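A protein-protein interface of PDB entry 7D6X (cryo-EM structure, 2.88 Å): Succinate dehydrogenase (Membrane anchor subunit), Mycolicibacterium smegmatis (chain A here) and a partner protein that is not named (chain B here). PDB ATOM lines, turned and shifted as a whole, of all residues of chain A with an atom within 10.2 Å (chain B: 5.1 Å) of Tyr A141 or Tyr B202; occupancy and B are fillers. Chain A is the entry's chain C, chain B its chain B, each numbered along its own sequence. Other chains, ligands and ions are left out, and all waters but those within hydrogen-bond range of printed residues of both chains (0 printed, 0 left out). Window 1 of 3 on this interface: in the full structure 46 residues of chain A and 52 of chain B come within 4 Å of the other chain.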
ATOM      1  N   THR A  11       3.120  -2.518  -8.149  1.00  0.00           N
ATOM      2  CA  THR A  11       2.555  -1.180  -8.050  1.00  0.00           C
ATOM      3  C   THR A  11       2.195  -0.709  -6.646  1.00  0.00           C
ATOM      4  O   THR A  11       2.804   0.240  -6.144  1.00  0.00           O
ATOM      5  CB  THR A  11       1.312  -1.078  -8.933  1.00  0.00           C
ATOM      6  OG1 THR A  11       0.346  -2.046  -8.512  1.00  0.00           O
ATOM      7  CG2 THR A  11       1.670  -1.318 -10.385  1.00  0.00           C
ATOM      8  N   ARG A 118     -22.054   8.108  -7.263  1.00  0.00           N
ATOM      9  CA  ARG A 118     -20.650   8.145  -7.644  1.00  0.00           C
ATOM     10  C   ARG A 118     -19.860   7.076  -6.914  1.00  0.00           C
ATOM     11  O   ARG A 118     -19.094   6.335  -7.531  1.00  0.00           O
ATOM     12  CB  ARG A 118     -20.068   9.527  -7.376  1.00  0.00           C
ATOM     13  CG  ARG A 118     -20.123  10.430  -8.573  1.00  0.00           C
ATOM     14  CD  ARG A 118     -20.374  11.847  -8.165  1.00  0.00           C
ATOM     15  NE  ARG A 118     -19.206  12.456  -7.558  1.00  0.00           N
ATOM     16  CZ  ARG A 118     -19.171  13.711  -7.142  1.00  0.00           C
ATOM     17  NH1 ARG A 118     -20.244  14.473  -7.271  1.00  0.00           N
ATOM     18  NH2 ARG A 118     -18.073  14.206  -6.602  1.00  0.00           N
ATOM     19  N   TYR A 122     -18.168   4.050  -8.968  1.00  0.00           N
ATOM     20  CA  TYR A 122     -16.717   4.007  -8.866  1.00  0.00           C
ATOM     21  C   TYR A 122     -16.256   2.674  -8.303  1.00  0.00           C
ATOM     22  O   TYR A 122     -15.236   2.135  -8.738  1.00  0.00           O
ATOM     23  CB  TYR A 122     -16.202   5.140  -7.984  1.00  0.00           C
ATOM     24  CG  TYR A 122     -16.256   6.513  -8.598  1.00  0.00           C
ATOM     25  CD1 TYR A 122     -16.168   6.690  -9.962  1.00  0.00           C
ATOM     26  CD2 TYR A 122     -16.388   7.635  -7.802  1.00  0.00           C
ATOM     27  CE1 TYR A 122     -16.220   7.943 -10.513  1.00  0.00           C
ATOM     28  CE2 TYR A 122     -16.442   8.888  -8.345  1.00  0.00           C
ATOM     29  CZ  TYR A 122     -16.356   9.037  -9.700  1.00  0.00           C
ATOM     30  OH  TYR A 122     -16.406  10.295 -10.244  1.00  0.00           O
ATOM     31  N   ARG A 123     -16.995   2.123  -7.341  1.00  0.00           N
ATOM     32  CA  ARG A 123     -16.646   0.801  -6.838  1.00  0.00           C
ATOM     33  C   ARG A 123     -16.998  -0.288  -7.842  1.00  0.00           C
ATOM     34  O   ARG A 123     -16.201  -1.198  -8.081  1.00  0.00           O
ATOM     35  CB  ARG A 123     -17.348   0.541  -5.514  1.00  0.00           C
ATOM     36  CG  ARG A 123     -16.774   1.280  -4.335  1.00  0.00           C
ATOM     37  CD  ARG A 123     -17.211   0.604  -3.063  1.00  0.00           C
ATOM     38  NE  ARG A 123     -16.820   1.334  -1.868  1.00  0.00           N
ATOM     39  CZ  ARG A 123     -16.912   0.839  -0.641  1.00  0.00           C
ATOM     40  NH1 ARG A 123     -17.374  -0.385  -0.460  1.00  0.00           N
ATOM     41  NH2 ARG A 123     -16.544   1.563   0.401  1.00  0.00           N
ATOM     42  N   TRP A 126     -15.933   1.182 -12.400  1.00  0.00           N
ATOM     43  CA  TRP A 126     -14.578   1.650 -12.650  1.00  0.00           C
ATOM     44  C   TRP A 126     -13.521   0.837 -11.928  1.00  0.00           C
ATOM     45  O   TRP A 126     -12.332   1.034 -12.191  1.00  0.00           O
ATOM     46  CB  TRP A 126     -14.444   3.119 -12.265  1.00  0.00           C
ATOM     47  CG  TRP A 126     -13.205   3.771 -12.804  1.00  0.00           C
ATOM     48  CD1 TRP A 126     -12.334   4.557 -12.114  1.00  0.00           C
ATOM     49  CD2 TRP A 126     -12.691   3.685 -14.144  1.00  0.00           C
ATOM     50  NE1 TRP A 126     -11.315   4.969 -12.934  1.00  0.00           N
ATOM     51  CE2 TRP A 126     -11.510   4.447 -14.184  1.00  0.00           C
ATOM     52  CE3 TRP A 126     -13.117   3.042 -15.311  1.00  0.00           C
ATOM     53  CZ2 TRP A 126     -10.751   4.583 -15.342  1.00  0.00           C
ATOM     54  CZ3 TRP A 126     -12.362   3.177 -16.455  1.00  0.00           C
ATOM     55  CH2 TRP A 126     -11.193   3.942 -16.463  1.00  0.00           C
ATOM     56  N   GLN A 127     -13.916  -0.056 -11.030  1.00  0.00           N
ATOM     57  CA  GLN A 127     -13.019  -0.950 -10.309  1.00  0.00           C
ATOM     58  C   GLN A 127     -12.041  -0.213  -9.411  1.00  0.00           C
ATOM     59  O   GLN A 127     -11.185  -0.849  -8.792  1.00  0.00           O
ATOM     60  CB  GLN A 127     -12.255  -1.876 -11.260  1.00  0.00           C
ATOM     61  CG  GLN A 127     -13.135  -2.838 -12.022  1.00  0.00           C
ATOM     62  CD  GLN A 127     -14.072  -3.591 -11.117  1.00  0.00           C
ATOM     63  OE1 GLN A 127     -13.691  -4.013 -10.028  1.00  0.00           O
ATOM     64  NE2 GLN A 127     -15.308  -3.770 -11.560  1.00  0.00           N
ATOM     65  N   SER A 128     -12.124   1.113  -9.334  1.00  0.00           N
ATOM     66  CA  SER A 128     -11.638   1.784  -8.145  1.00  0.00           C
ATOM     67  C   SER A 128     -12.326   1.118  -6.960  1.00  0.00           C
ATOM     68  O   SER A 128     -13.470   0.675  -7.090  1.00  0.00           O
ATOM     69  CB  SER A 128     -11.942   3.274  -8.193  1.00  0.00           C
ATOM     70  OG  SER A 128     -10.994   3.939  -8.998  1.00  0.00           O
ATOM     71  N   PRO A 129     -11.710   1.112  -5.790  1.00  0.00           N
ATOM     72  CA  PRO A 129     -11.660  -0.126  -5.005  1.00  0.00           C
ATOM     73  C   PRO A 129     -12.931  -0.948  -5.090  1.00  0.00           C
ATOM     74  O   PRO A 129     -14.002  -0.483  -4.695  1.00  0.00           O
ATOM     75  CB  PRO A 129     -11.430   0.384  -3.580  1.00  0.00           C
ATOM     76  CG  PRO A 129     -12.034   1.717  -3.588  1.00  0.00           C
ATOM     77  CD  PRO A 129     -11.672   2.289  -4.916  1.00  0.00           C
ATOM     78  N   GLU A 136      -6.397  -2.732  -6.187  1.00  0.00           N
ATOM     79  CA  GLU A 136      -7.003  -2.117  -7.355  1.00  0.00           C
ATOM     80  C   GLU A 136      -6.325  -2.619  -8.628  1.00  0.00           C
ATOM     81  O   GLU A 136      -5.102  -2.778  -8.659  1.00  0.00           O
ATOM     82  CB  GLU A 136      -6.878  -0.597  -7.247  1.00  0.00           C
ATOM     83  CG  GLU A 136      -7.857   0.201  -8.066  1.00  0.00           C
ATOM     84  CD  GLU A 136      -7.743   1.689  -7.801  1.00  0.00           C
ATOM     85  OE1 GLU A 136      -7.583   2.074  -6.625  1.00  0.00           O
ATOM     86  OE2 GLU A 136      -7.805   2.475  -8.767  1.00  0.00           O
ATOM     87  N   PRO A 137      -7.088  -2.888  -9.692  1.00  0.00           N
ATOM     88  CA  PRO A 137      -6.476  -3.370 -10.938  1.00  0.00           C
ATOM     89  C   PRO A 137      -5.832  -2.288 -11.791  1.00  0.00           C
ATOM     90  O   PRO A 137      -5.173  -2.625 -12.783  1.00  0.00           O
ATOM     91  CB  PRO A 137      -7.659  -4.008 -11.677  1.00  0.00           C
ATOM     92  CG  PRO A 137      -8.843  -3.294 -11.170  1.00  0.00           C
ATOM     93  CD  PRO A 137      -8.558  -2.952  -9.739  1.00  0.00           C
ATOM     94  N   HIS A 138      -5.990  -1.013 -11.446  1.00  0.00           N
ATOM     95  CA  HIS A 138      -5.454   0.081 -12.241  1.00  0.00           C
ATOM     96  C   HIS A 138      -4.058   0.456 -11.768  1.00  0.00           C
ATOM     97  O   HIS A 138      -3.757   0.396 -10.574  1.00  0.00           O
ATOM     98  CB  HIS A 138      -6.365   1.303 -12.155  1.00  0.00           C
ATOM     99  CG  HIS A 138      -7.783   1.031 -12.546  1.00  0.00           C
ATOM    100  ND1 HIS A 138      -8.191   0.953 -13.859  1.00  0.00           N
ATOM    101  CD2 HIS A 138      -8.891   0.838 -11.796  1.00  0.00           C
ATOM    102  CE1 HIS A 138      -9.489   0.716 -13.901  1.00  0.00           C
ATOM    103  NE2 HIS A 138      -9.938   0.641 -12.662  1.00  0.00           N
ATOM    104  N   ALA A 139      -3.210   0.857 -12.714  1.00  0.00           N
ATOM    105  CA  ALA A 139      -1.838   1.214 -12.377  1.00  0.00           C
ATOM    106  C   ALA A 139      -1.714   2.681 -11.983  1.00  0.00           C
ATOM    107  O   ALA A 139      -1.059   3.004 -10.987  1.00  0.00           O
ATOM    108  CB  ALA A 139      -0.913   0.897 -13.548  1.00  0.00           C
ATOM    109  N   LYS A 140      -2.335   3.577 -12.744  1.00  0.00           N
ATOM    110  CA  LYS A 140      -2.298   5.007 -12.480  1.00  0.00           C
ATOM    111  C   LYS A 140      -3.687   5.503 -12.107  1.00  0.00           C
ATOM    112  O   LYS A 140      -4.698   4.960 -12.557  1.00  0.00           O
ATOM    113  CB  LYS A 140      -1.770   5.777 -13.690  1.00  0.00           C
ATOM    114  CG  LYS A 140      -2.627   5.625 -14.925  1.00  0.00           C
ATOM    115  CD  LYS A 140      -1.997   6.305 -16.125  1.00  0.00           C
ATOM    116  CE  LYS A 140      -2.859   6.136 -17.366  1.00  0.00           C
ATOM    117  NZ  LYS A 140      -2.909   4.719 -17.817  1.00  0.00           N
ATOM    118  N   TYR A 141      -3.724   6.540 -11.276  1.00  0.00           N
ATOM    119  CA  TYR A 141      -4.966   7.071 -10.737  1.00  0.00           C
ATOM    120  C   TYR A 141      -4.825   8.572 -10.567  1.00  0.00           C
ATOM    121  O   TYR A 141      -3.813   9.043 -10.042  1.00  0.00           O
ATOM    122  CB  TYR A 141      -5.298   6.415  -9.400  1.00  0.00           C
ATOM    123  CG  TYR A 141      -6.460   7.011  -8.650  1.00  0.00           C
ATOM    124  CD1 TYR A 141      -7.761   6.634  -8.932  1.00  0.00           C
ATOM    125  CD2 TYR A 141      -6.253   7.918  -7.632  1.00  0.00           C
ATOM    126  CE1 TYR A 141      -8.817   7.163  -8.239  1.00  0.00           C
ATOM    127  CE2 TYR A 141      -7.304   8.450  -6.935  1.00  0.00           C
ATOM    128  CZ  TYR A 141      -8.581   8.069  -7.239  1.00  0.00           C
ATOM    129  OH  TYR A 141      -9.624   8.610  -6.539  1.00  0.00           O
ATOM    130  N   THR A 142      -5.828   9.319 -11.023  1.00  0.00           N
ATOM    131  CA  THR A 142      -5.835  10.768 -10.897  1.00  0.00           C
ATOM    132  C   THR A 142      -7.054  11.299 -10.164  1.00  0.00           C
ATOM    133  O   THR A 142      -7.153  12.511  -9.966  1.00  0.00           O
ATOM    134  CB  THR A 142      -5.754  11.429 -12.276  1.00  0.00           C
ATOM    135  OG1 THR A 142      -6.965  11.185 -12.994  1.00  0.00           O
ATOM    136  CG2 THR A 142      -4.590  10.869 -13.063  1.00  0.00           C
ATOM    137  N   GLY A 143      -7.980  10.437  -9.759  1.00  0.00           N
ATOM    138  CA  GLY A 143      -9.141  10.876  -9.016  1.00  0.00           C
ATOM    139  C   GLY A 143     -10.034  11.782  -9.839  1.00  0.00           C
ATOM    140  O   GLY A 143     -10.079  11.716 -11.069  1.00  0.00           O
ATOM    141  N   GLU A 144     -10.755  12.650  -9.141  1.00  0.00           N
ATOM    142  CA  GLU A 144     -11.588  13.658  -9.787  1.00  0.00           C
ATOM    143  C   GLU A 144     -10.823  14.956  -9.997  1.00  0.00           C
ATOM    144  O   GLU A 144     -11.287  16.033  -9.636  1.00  0.00           O
ATOM    145  CB  GLU A 144     -12.843  13.891  -8.959  1.00  0.00           C
ATOM    146  CG  GLU A 144     -13.745  12.676  -8.868  1.00  0.00           C
ATOM    147  CD  GLU A 144     -14.990  12.934  -8.058  1.00  0.00           C
ATOM    148  OE1 GLU A 144     -15.103  14.031  -7.478  1.00  0.00           O
ATOM    149  OE2 GLU A 144     -15.857  12.041  -8.002  1.00  0.00           O
ATOM    150  N   THR A 145      -9.637  14.863 -10.590  1.00  0.00           N
ATOM    151  CA  THR A 145      -8.794  16.026 -10.815  1.00  0.00           C
ATOM    152  C   THR A 145      -8.596  16.369 -12.279  1.00  0.00           C
ATOM    153  O   THR A 145      -8.350  17.535 -12.590  1.00  0.00           O
ATOM    154  CB  THR A 145      -7.411  15.833 -10.172  1.00  0.00           C
ATOM    155  OG1 THR A 145      -6.681  14.835 -10.888  1.00  0.00           O
ATOM    156  CG2 THR A 145      -7.541  15.403  -8.737  1.00  0.00           C
ATOM    157  N   ARG A 146      -8.691  15.400 -13.182  1.00  0.00           N
ATOM    158  CA  ARG A 146      -8.504  15.653 -14.601  1.00  0.00           C
ATOM    159  C   ARG A 146      -9.843  16.038 -15.224  1.00  0.00           C
ATOM    160  O   ARG A 146     -10.822  16.283 -14.520  1.00  0.00           O
ATOM    161  CB  ARG A 146      -7.869  14.442 -15.275  1.00  0.00           C
ATOM    162  CG  ARG A 146      -6.535  14.050 -14.686  1.00  0.00           C
ATOM    163  CD  ARG A 146      -5.625  15.246 -14.558  1.00  0.00           C
ATOM    164  NE  ARG A 146      -5.128  15.682 -15.856  1.00  0.00           N
ATOM    165  CZ  ARG A 146      -3.937  15.355 -16.344  1.00  0.00           C
ATOM    166  NH1 ARG A 146      -3.562  15.794 -17.538  1.00  0.00           N
ATOM    167  NH2 ARG A 146      -3.117  14.588 -15.637  1.00  0.00           N
ATOM    168  N   LEU A 149     -13.770  14.024 -15.080  1.00  0.00           N
ATOM    169  CA  LEU A 149     -14.275  13.821 -13.734  1.00  0.00           C
ATOM    170  C   LEU A 149     -14.206  15.069 -12.869  1.00  0.00           C
ATOM    171  O   LEU A 149     -14.722  15.051 -11.750  1.00  0.00           O
ATOM    172  CB  LEU A 149     -13.516  12.680 -13.053  1.00  0.00           C
ATOM    173  CG  LEU A 149     -14.221  11.323 -13.038  1.00  0.00           C
ATOM    174  CD1 LEU A 149     -14.671  10.928 -14.425  1.00  0.00           C
ATOM    175  CD2 LEU A 149     -13.316  10.259 -12.455  1.00  0.00           C
ATOM    176  N   ILE A 150     -13.587  16.149 -13.348  1.00  0.00           N
ATOM    177  CA  ILE A 150     -13.683  17.425 -12.650  1.00  0.00           C
ATOM    178  C   ILE A 150     -15.069  18.029 -12.783  1.00  0.00           C
ATOM    179  O   ILE A 150     -15.416  18.943 -12.031  1.00  0.00           O
ATOM    180  CB  ILE A 150     -12.615  18.413 -13.166  1.00  0.00           C
ATOM    181  CG1 ILE A 150     -12.302  19.483 -12.125  1.00  0.00           C
ATOM    182  CG2 ILE A 150     -13.055  19.068 -14.450  1.00  0.00           C
ATOM    183  CD1 ILE A 150     -11.602  18.966 -10.917  1.00  0.00           C
ATOM    184  N   ASN A 153     -18.408  18.255  -9.976  1.00  0.00           N
ATOM    185  CA  ASN A 153     -18.631  19.294  -8.985  1.00  0.00           C
ATOM    186  C   ASN A 153     -19.801  20.196  -9.330  1.00  0.00           C
ATOM    187  O   ASN A 153     -20.085  21.131  -8.573  1.00  0.00           O
ATOM    188  CB  ASN A 153     -17.368  20.137  -8.823  1.00  0.00           C
ATOM    189  CG  ASN A 153     -16.144  19.299  -8.562  1.00  0.00           C
ATOM    190  OD1 ASN A 153     -15.921  18.839  -7.447  1.00  0.00           O
ATOM    191  ND2 ASN A 153     -15.340  19.094  -9.593  1.00  0.00           N
ATOM    192  N   HIS B 156      -7.487   3.824  -1.014  1.00  0.00           N
ATOM    193  CA  HIS B 156      -6.856   3.295  -2.214  1.00  0.00           C
ATOM    194  C   HIS B 156      -5.979   4.312  -2.923  1.00  0.00           C
ATOM    195  O   HIS B 156      -5.165   3.923  -3.764  1.00  0.00           O
ATOM    196  CB  HIS B 156      -7.919   2.800  -3.184  1.00  0.00           C
ATOM    197  CG  HIS B 156      -8.773   3.892  -3.743  1.00  0.00           C
ATOM    198  ND1 HIS B 156      -8.686   4.305  -5.052  1.00  0.00           N
ATOM    199  CD2 HIS B 156      -9.729   4.654  -3.169  1.00  0.00           C
ATOM    200  CE1 HIS B 156      -9.553   5.278  -5.261  1.00  0.00           C
ATOM    201  NE2 HIS B 156     -10.199   5.508  -4.134  1.00  0.00           N
ATOM    202  N   VAL B 157      -6.143   5.602  -2.637  1.00  0.00           N
ATOM    203  CA  VAL B 157      -5.342   6.612  -3.318  1.00  0.00           C
ATOM    204  C   VAL B 157      -3.873   6.439  -2.974  1.00  0.00           C
ATOM    205  O   VAL B 157      -2.997   6.578  -3.835  1.00  0.00           O
ATOM    206  CB  VAL B 157      -5.844   8.020  -2.960  1.00  0.00           C
ATOM    207  CG1 VAL B 157      -5.115   9.056  -3.767  1.00  0.00           C
ATOM    208  CG2 VAL B 157      -7.324   8.120  -3.192  1.00  0.00           C
ATOM    209  N   HIS B 161      -1.395   3.188  -4.923  1.00  0.00           N
ATOM    210  CA  HIS B 161      -0.571   4.015  -5.799  1.00  0.00           C
ATOM    211  C   HIS B 161       0.464   4.721  -4.939  1.00  0.00           C
ATOM    212  O   HIS B 161       0.112   5.546  -4.093  1.00  0.00           O
ATOM    213  CB  HIS B 161      -1.421   5.020  -6.569  1.00  0.00           C
ATOM    214  CG  HIS B 161      -2.642   4.420  -7.190  1.00  0.00           C
ATOM    215  ND1 HIS B 161      -2.617   3.779  -8.407  1.00  0.00           N
ATOM    216  CD2 HIS B 161      -3.921   4.358  -6.757  1.00  0.00           C
ATOM    217  CE1 HIS B 161      -3.830   3.348  -8.698  1.00  0.00           C
ATOM    218  NE2 HIS B 161      -4.639   3.685  -7.712  1.00  0.00           N
ATOM    219  N   GLU B 163       2.953   6.721  -6.042  1.00  0.00           N
ATOM    220  CA  GLU B 163       3.263   8.054  -6.534  1.00  0.00           C
ATOM    221  C   GLU B 163       2.281   9.109  -6.050  1.00  0.00           C
ATOM    222  O   GLU B 163       2.552  10.298  -6.224  1.00  0.00           O
ATOM    223  CB  GLU B 163       3.305   8.045  -8.059  1.00  0.00           C
ATOM    224  CG  GLU B 163       1.947   7.921  -8.718  1.00  0.00           C
ATOM    225  CD  GLU B 163       1.517   6.483  -8.919  1.00  0.00           C
ATOM    226  OE1 GLU B 163       0.307   6.246  -9.113  1.00  0.00           O
ATOM    227  OE2 GLU B 163       2.385   5.591  -8.884  1.00  0.00           O
ATOM    228  N   ASN B 164       1.159   8.712  -5.457  1.00  0.00           N
ATOM    229  CA  ASN B 164       0.196   9.651  -4.904  1.00  0.00           C
ATOM    230  C   ASN B 164       0.449   9.965  -3.439  1.00  0.00           C
ATOM    231  O   ASN B 164      -0.328  10.710  -2.843  1.00  0.00           O
ATOM    232  CB  ASN B 164      -1.226   9.117  -5.052  1.00  0.00           C
ATOM    233  CG  ASN B 164      -1.613   8.882  -6.485  1.00  0.00           C
ATOM    234  OD1 ASN B 164      -0.944   9.339  -7.403  1.00  0.00           O
ATOM    235  ND2 ASN B 164      -2.706   8.168  -6.687  1.00  0.00           N
ATOM    236  N   ASN B 167       1.132  13.692  -3.201  1.00  0.00           N
ATOM    237  CA  ASN B 167       0.078  14.604  -3.617  1.00  0.00           C
ATOM    238  C   ASN B 167      -1.156  14.556  -2.737  1.00  0.00           C
ATOM    239  O   ASN B 167      -1.902  15.534  -2.698  1.00  0.00           O
ATOM    240  CB  ASN B 167      -0.340  14.300  -5.056  1.00  0.00           C
ATOM    241  CG  ASN B 167       0.838  14.101  -5.971  1.00  0.00           C
ATOM    242  OD1 ASN B 167       1.867  14.753  -5.824  1.00  0.00           O
ATOM    243  ND2 ASN B 167       0.696  13.192  -6.925  1.00  0.00           N
ATOM    244  N   PHE B 168      -1.396  13.449  -2.049  1.00  0.00           N
ATOM    245  CA  PHE B 168      -2.577  13.270  -1.222  1.00  0.00           C
ATOM    246  C   PHE B 168      -2.172  13.243   0.244  1.00  0.00           C
ATOM    247  O   PHE B 168      -1.183  12.605   0.610  1.00  0.00           O
ATOM    248  CB  PHE B 168      -3.304  11.977  -1.591  1.00  0.00           C
ATOM    249  CG  PHE B 168      -4.703  11.895  -1.073  1.00  0.00           C
ATOM    250  CD1 PHE B 168      -5.579  12.937  -1.254  1.00  0.00           C
ATOM    251  CD2 PHE B 168      -5.144  10.769  -0.416  1.00  0.00           C
ATOM    252  CE1 PHE B 168      -6.863  12.864  -0.785  1.00  0.00           C
ATOM    253  CE2 PHE B 168      -6.429  10.694   0.054  1.00  0.00           C
ATOM    254  CZ  PHE B 168      -7.287  11.743  -0.131  1.00  0.00           C
ATOM    255  N   GLY B 199      -4.252  17.935  -2.378  1.00  0.00           N
ATOM    256  CA  GLY B 199      -4.937  17.077  -3.322  1.00  0.00           C
ATOM    257  C   GLY B 199      -6.253  16.494  -2.862  1.00  0.00           C
ATOM    258  O   GLY B 199      -6.433  15.278  -2.914  1.00  0.00           O
ATOM    259  N   LEU B 200      -7.183  17.336  -2.415  1.00  0.00           N
ATOM    260  CA  LEU B 200      -8.492  16.829  -2.019  1.00  0.00           C
ATOM    261  C   LEU B 200      -9.231  16.225  -3.199  1.00  0.00           C
ATOM    262  O   LEU B 200     -10.084  15.352  -3.016  1.00  0.00           O
ATOM    263  CB  LEU B 200      -9.317  17.946  -1.387  1.00  0.00           C
ATOM    264  CG  LEU B 200     -10.800  17.722  -1.093  1.00  0.00           C
ATOM    265  CD1 LEU B 200     -11.004  16.700   0.000  1.00  0.00           C
ATOM    266  CD2 LEU B 200     -11.442  19.028  -0.716  1.00  0.00           C
ATOM    267  N   GLY B 201      -8.915  16.659  -4.415  1.00  0.00           N
ATOM    268  CA  GLY B 201      -9.571  16.127  -5.591  1.00  0.00           C
ATOM    269  C   GLY B 201      -9.235  14.690  -5.902  1.00  0.00           C
ATOM    270  O   GLY B 201      -9.878  14.101  -6.775  1.00  0.00           O
ATOM    271  N   TYR B 202      -8.332  14.049  -5.238  1.00  0.00           N
ATOM    272  CA  TYR B 202      -7.985  12.715  -5.515  1.00  0.00           C
ATOM    273  C   TYR B 202      -8.843  11.761  -4.816  1.00  0.00           C
ATOM    274  O   TYR B 202      -8.689  10.581  -4.992  1.00  0.00           O
ATOM    275  CB  TYR B 202      -6.589  12.463  -5.115  1.00  0.00           C
ATOM    276  CG  TYR B 202      -5.481  12.893  -6.023  1.00  0.00           C
ATOM    277  CD1 TYR B 202      -4.856  14.107  -5.846  1.00  0.00           C
ATOM    278  CD2 TYR B 202      -5.005  12.051  -7.004  1.00  0.00           C
ATOM    279  CE1 TYR B 202      -3.819  14.494  -6.659  1.00  0.00           C
ATOM    280  CE2 TYR B 202      -3.968  12.428  -7.821  1.00  0.00           C
ATOM    281  CZ  TYR B 202      -3.384  13.652  -7.643  1.00  0.00           C
ATOM    282  OH  TYR B 202      -2.353  14.035  -8.457  1.00  0.00           O
ATOM    283  N   CYS B 203      -9.762  12.214  -4.017  1.00  0.00           N
ATOM    284  CA  CYS B 203     -10.633  11.370  -3.347  1.00  0.00           C
ATOM    285  C   CYS B 203     -11.872  11.232  -4.038  1.00  0.00           C
ATOM    286  O   CYS B 203     -12.619  12.172  -4.170  1.00  0.00           O
ATOM    287  CB  CYS B 203     -11.074  11.946  -2.043  1.00  0.00           C
ATOM    288  SG  CYS B 203     -12.116  10.895  -1.007  1.00  0.00           S
ATOM    289  N   ASN B 204     -12.095  10.049  -4.556  1.00  0.00           N
ATOM    290  CA  ASN B 204     -13.454   9.727  -4.934  1.00  0.00           C
ATOM    291  C   ASN B 204     -14.203   9.272  -3.689  1.00  0.00           C
ATOM    292  O   ASN B 204     -13.615   8.790  -2.723  1.00  0.00           O
ATOM    293  CB  ASN B 204     -13.490   8.659  -6.021  1.00  0.00           C
ATOM    294  CG  ASN B 204     -12.652   7.457  -5.688  1.00  0.00           C
ATOM    295  OD1 ASN B 204     -12.142   7.329  -4.583  1.00  0.00           O
ATOM    296  ND2 ASN B 204     -12.516   6.554  -6.643  1.00  0.00           N
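Printed residues of chain A that touch a printed residue of chain B: Tyr A122, Ser A128, Pro A129, Glu A136, His A138, Ala A139, Tyr A141, Thr A142, Gly A143, Glu A144 and Thr A145. Among the printed residues, no Asp or Glu carboxylate lies within 4 Å of a Lys or Arg side-chain nitrogen of the other chain.
Tyr A141 touches just these residues of chain B: His B156 (3.6 Å), Val B157 (3.8 Å), His B161 (3.3 Å), Asn B164 (3.6 Å), Tyr B202 (2.7 Å) and Asn B204 (3.3 Å). Tyr B202 touches just these residues of chain A: Tyr A141 (2.7 Å), Thr A142 (3.7 Å) and Thr A145 (3.8 Å). Of chain A, only Tyr A141 comes within 4 Å of Val B157. No residue of chain A comes within 4 Å of Asn B167. No residue of chain A comes within 4 Å of Gly B199. Gly B201 touches just these residues of chain A: Gly A143, Glu A144 and Thr A145. Cys B203 touches none of the printed residues of chain A. Of chain A, only Tyr A122 (3.6 Å), Ser A128 (3.7 Å) and Tyr A141 (3.3 Å) come within 4 Å of Asn B204. Of the printed residues of chain A, Asn B164 touches Tyr A141 (3.6 Å). Printed residues of chain B within 4 Å of Ser A128: Asn B204 (3.7 Å). Printed residues of chain B within 4 Å of His A138: His B161 (3.5 Å). Printed residues of chain B within 4 Å of Glu A136: His B156 and His B161. Printed residues of chain B within 4 Å of Pro A129: His B156 (3.5 Å). Leu A149 touches none of the printed residues of chain B. Arg A123 touches none of the printed residues of chain B. The nearest residue of chain B that does not touch Tyr A141 is Cys B203 (4.3 Å). The nearest printed residue of chain A that does not touch Glu B163 is Lys A140 (4.4 Å).
The backbone carbonyl oxygen (O) of Tyr A122 is in hydrogen-bond range of the backbone NH (N) of Ser A128, 3.3 Å away. O of Val B157 sits at hydrogen-bond distance from ND2 of Asn B164, at 3.3 Å. O of Trp A126 sits at hydrogen-bond distance from NE2 of His A138. OD1 of Asn B204 sits at hydrogen-bond distance from NE2 of His B156, at 2.7 Å. OH of Tyr A122 lies within hydrogen-bond range of OE2 of Glu A144 (2.9 Å). The backbone carbonyl oxygen of Tyr A122 sits at hydrogen-bond distance from the backbone NH of Gln A127 (3.4 Å).
OE1 of Glu A136 lies within hydrogen-bond range of ND1 of His B156 (2.9 Å). The backbone carbonyl oxygen (O) of Tyr B202 sits at hydrogen-bond distance from the side-chain hydroxyl (OH) of Tyr A141, at 2.7 Å. The side-chain amide oxygen of Asn B204 sits close to the side-chain hydroxyl of Tyr A141 (3.4 Å). A ring nitrogen (ND1) of His B161 lies within hydrogen-bond range of the backbone carbonyl oxygen of Ala A139 (3.1 Å). O of Gly B201 lies within hydrogen-bond range of N of Glu A144 (2.9 Å).
Among the printed residues, merely in contact across the chains: Tyr A122 with Asn B204, Ser A128 with Asn B204, Pro A129 with His B156, Glu A136 with His B161, His A138 with His B161, Ala A139 with Glu B163, Tyr A141 with His B156, Tyr A141 with Val B157, Tyr A141 with His B161, Tyr A141 with Asn B164, Thr A142 with Tyr B202, Gly A143 with Gly B201, Thr A145 with Gly B201 and Thr A145 with Tyr B202.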
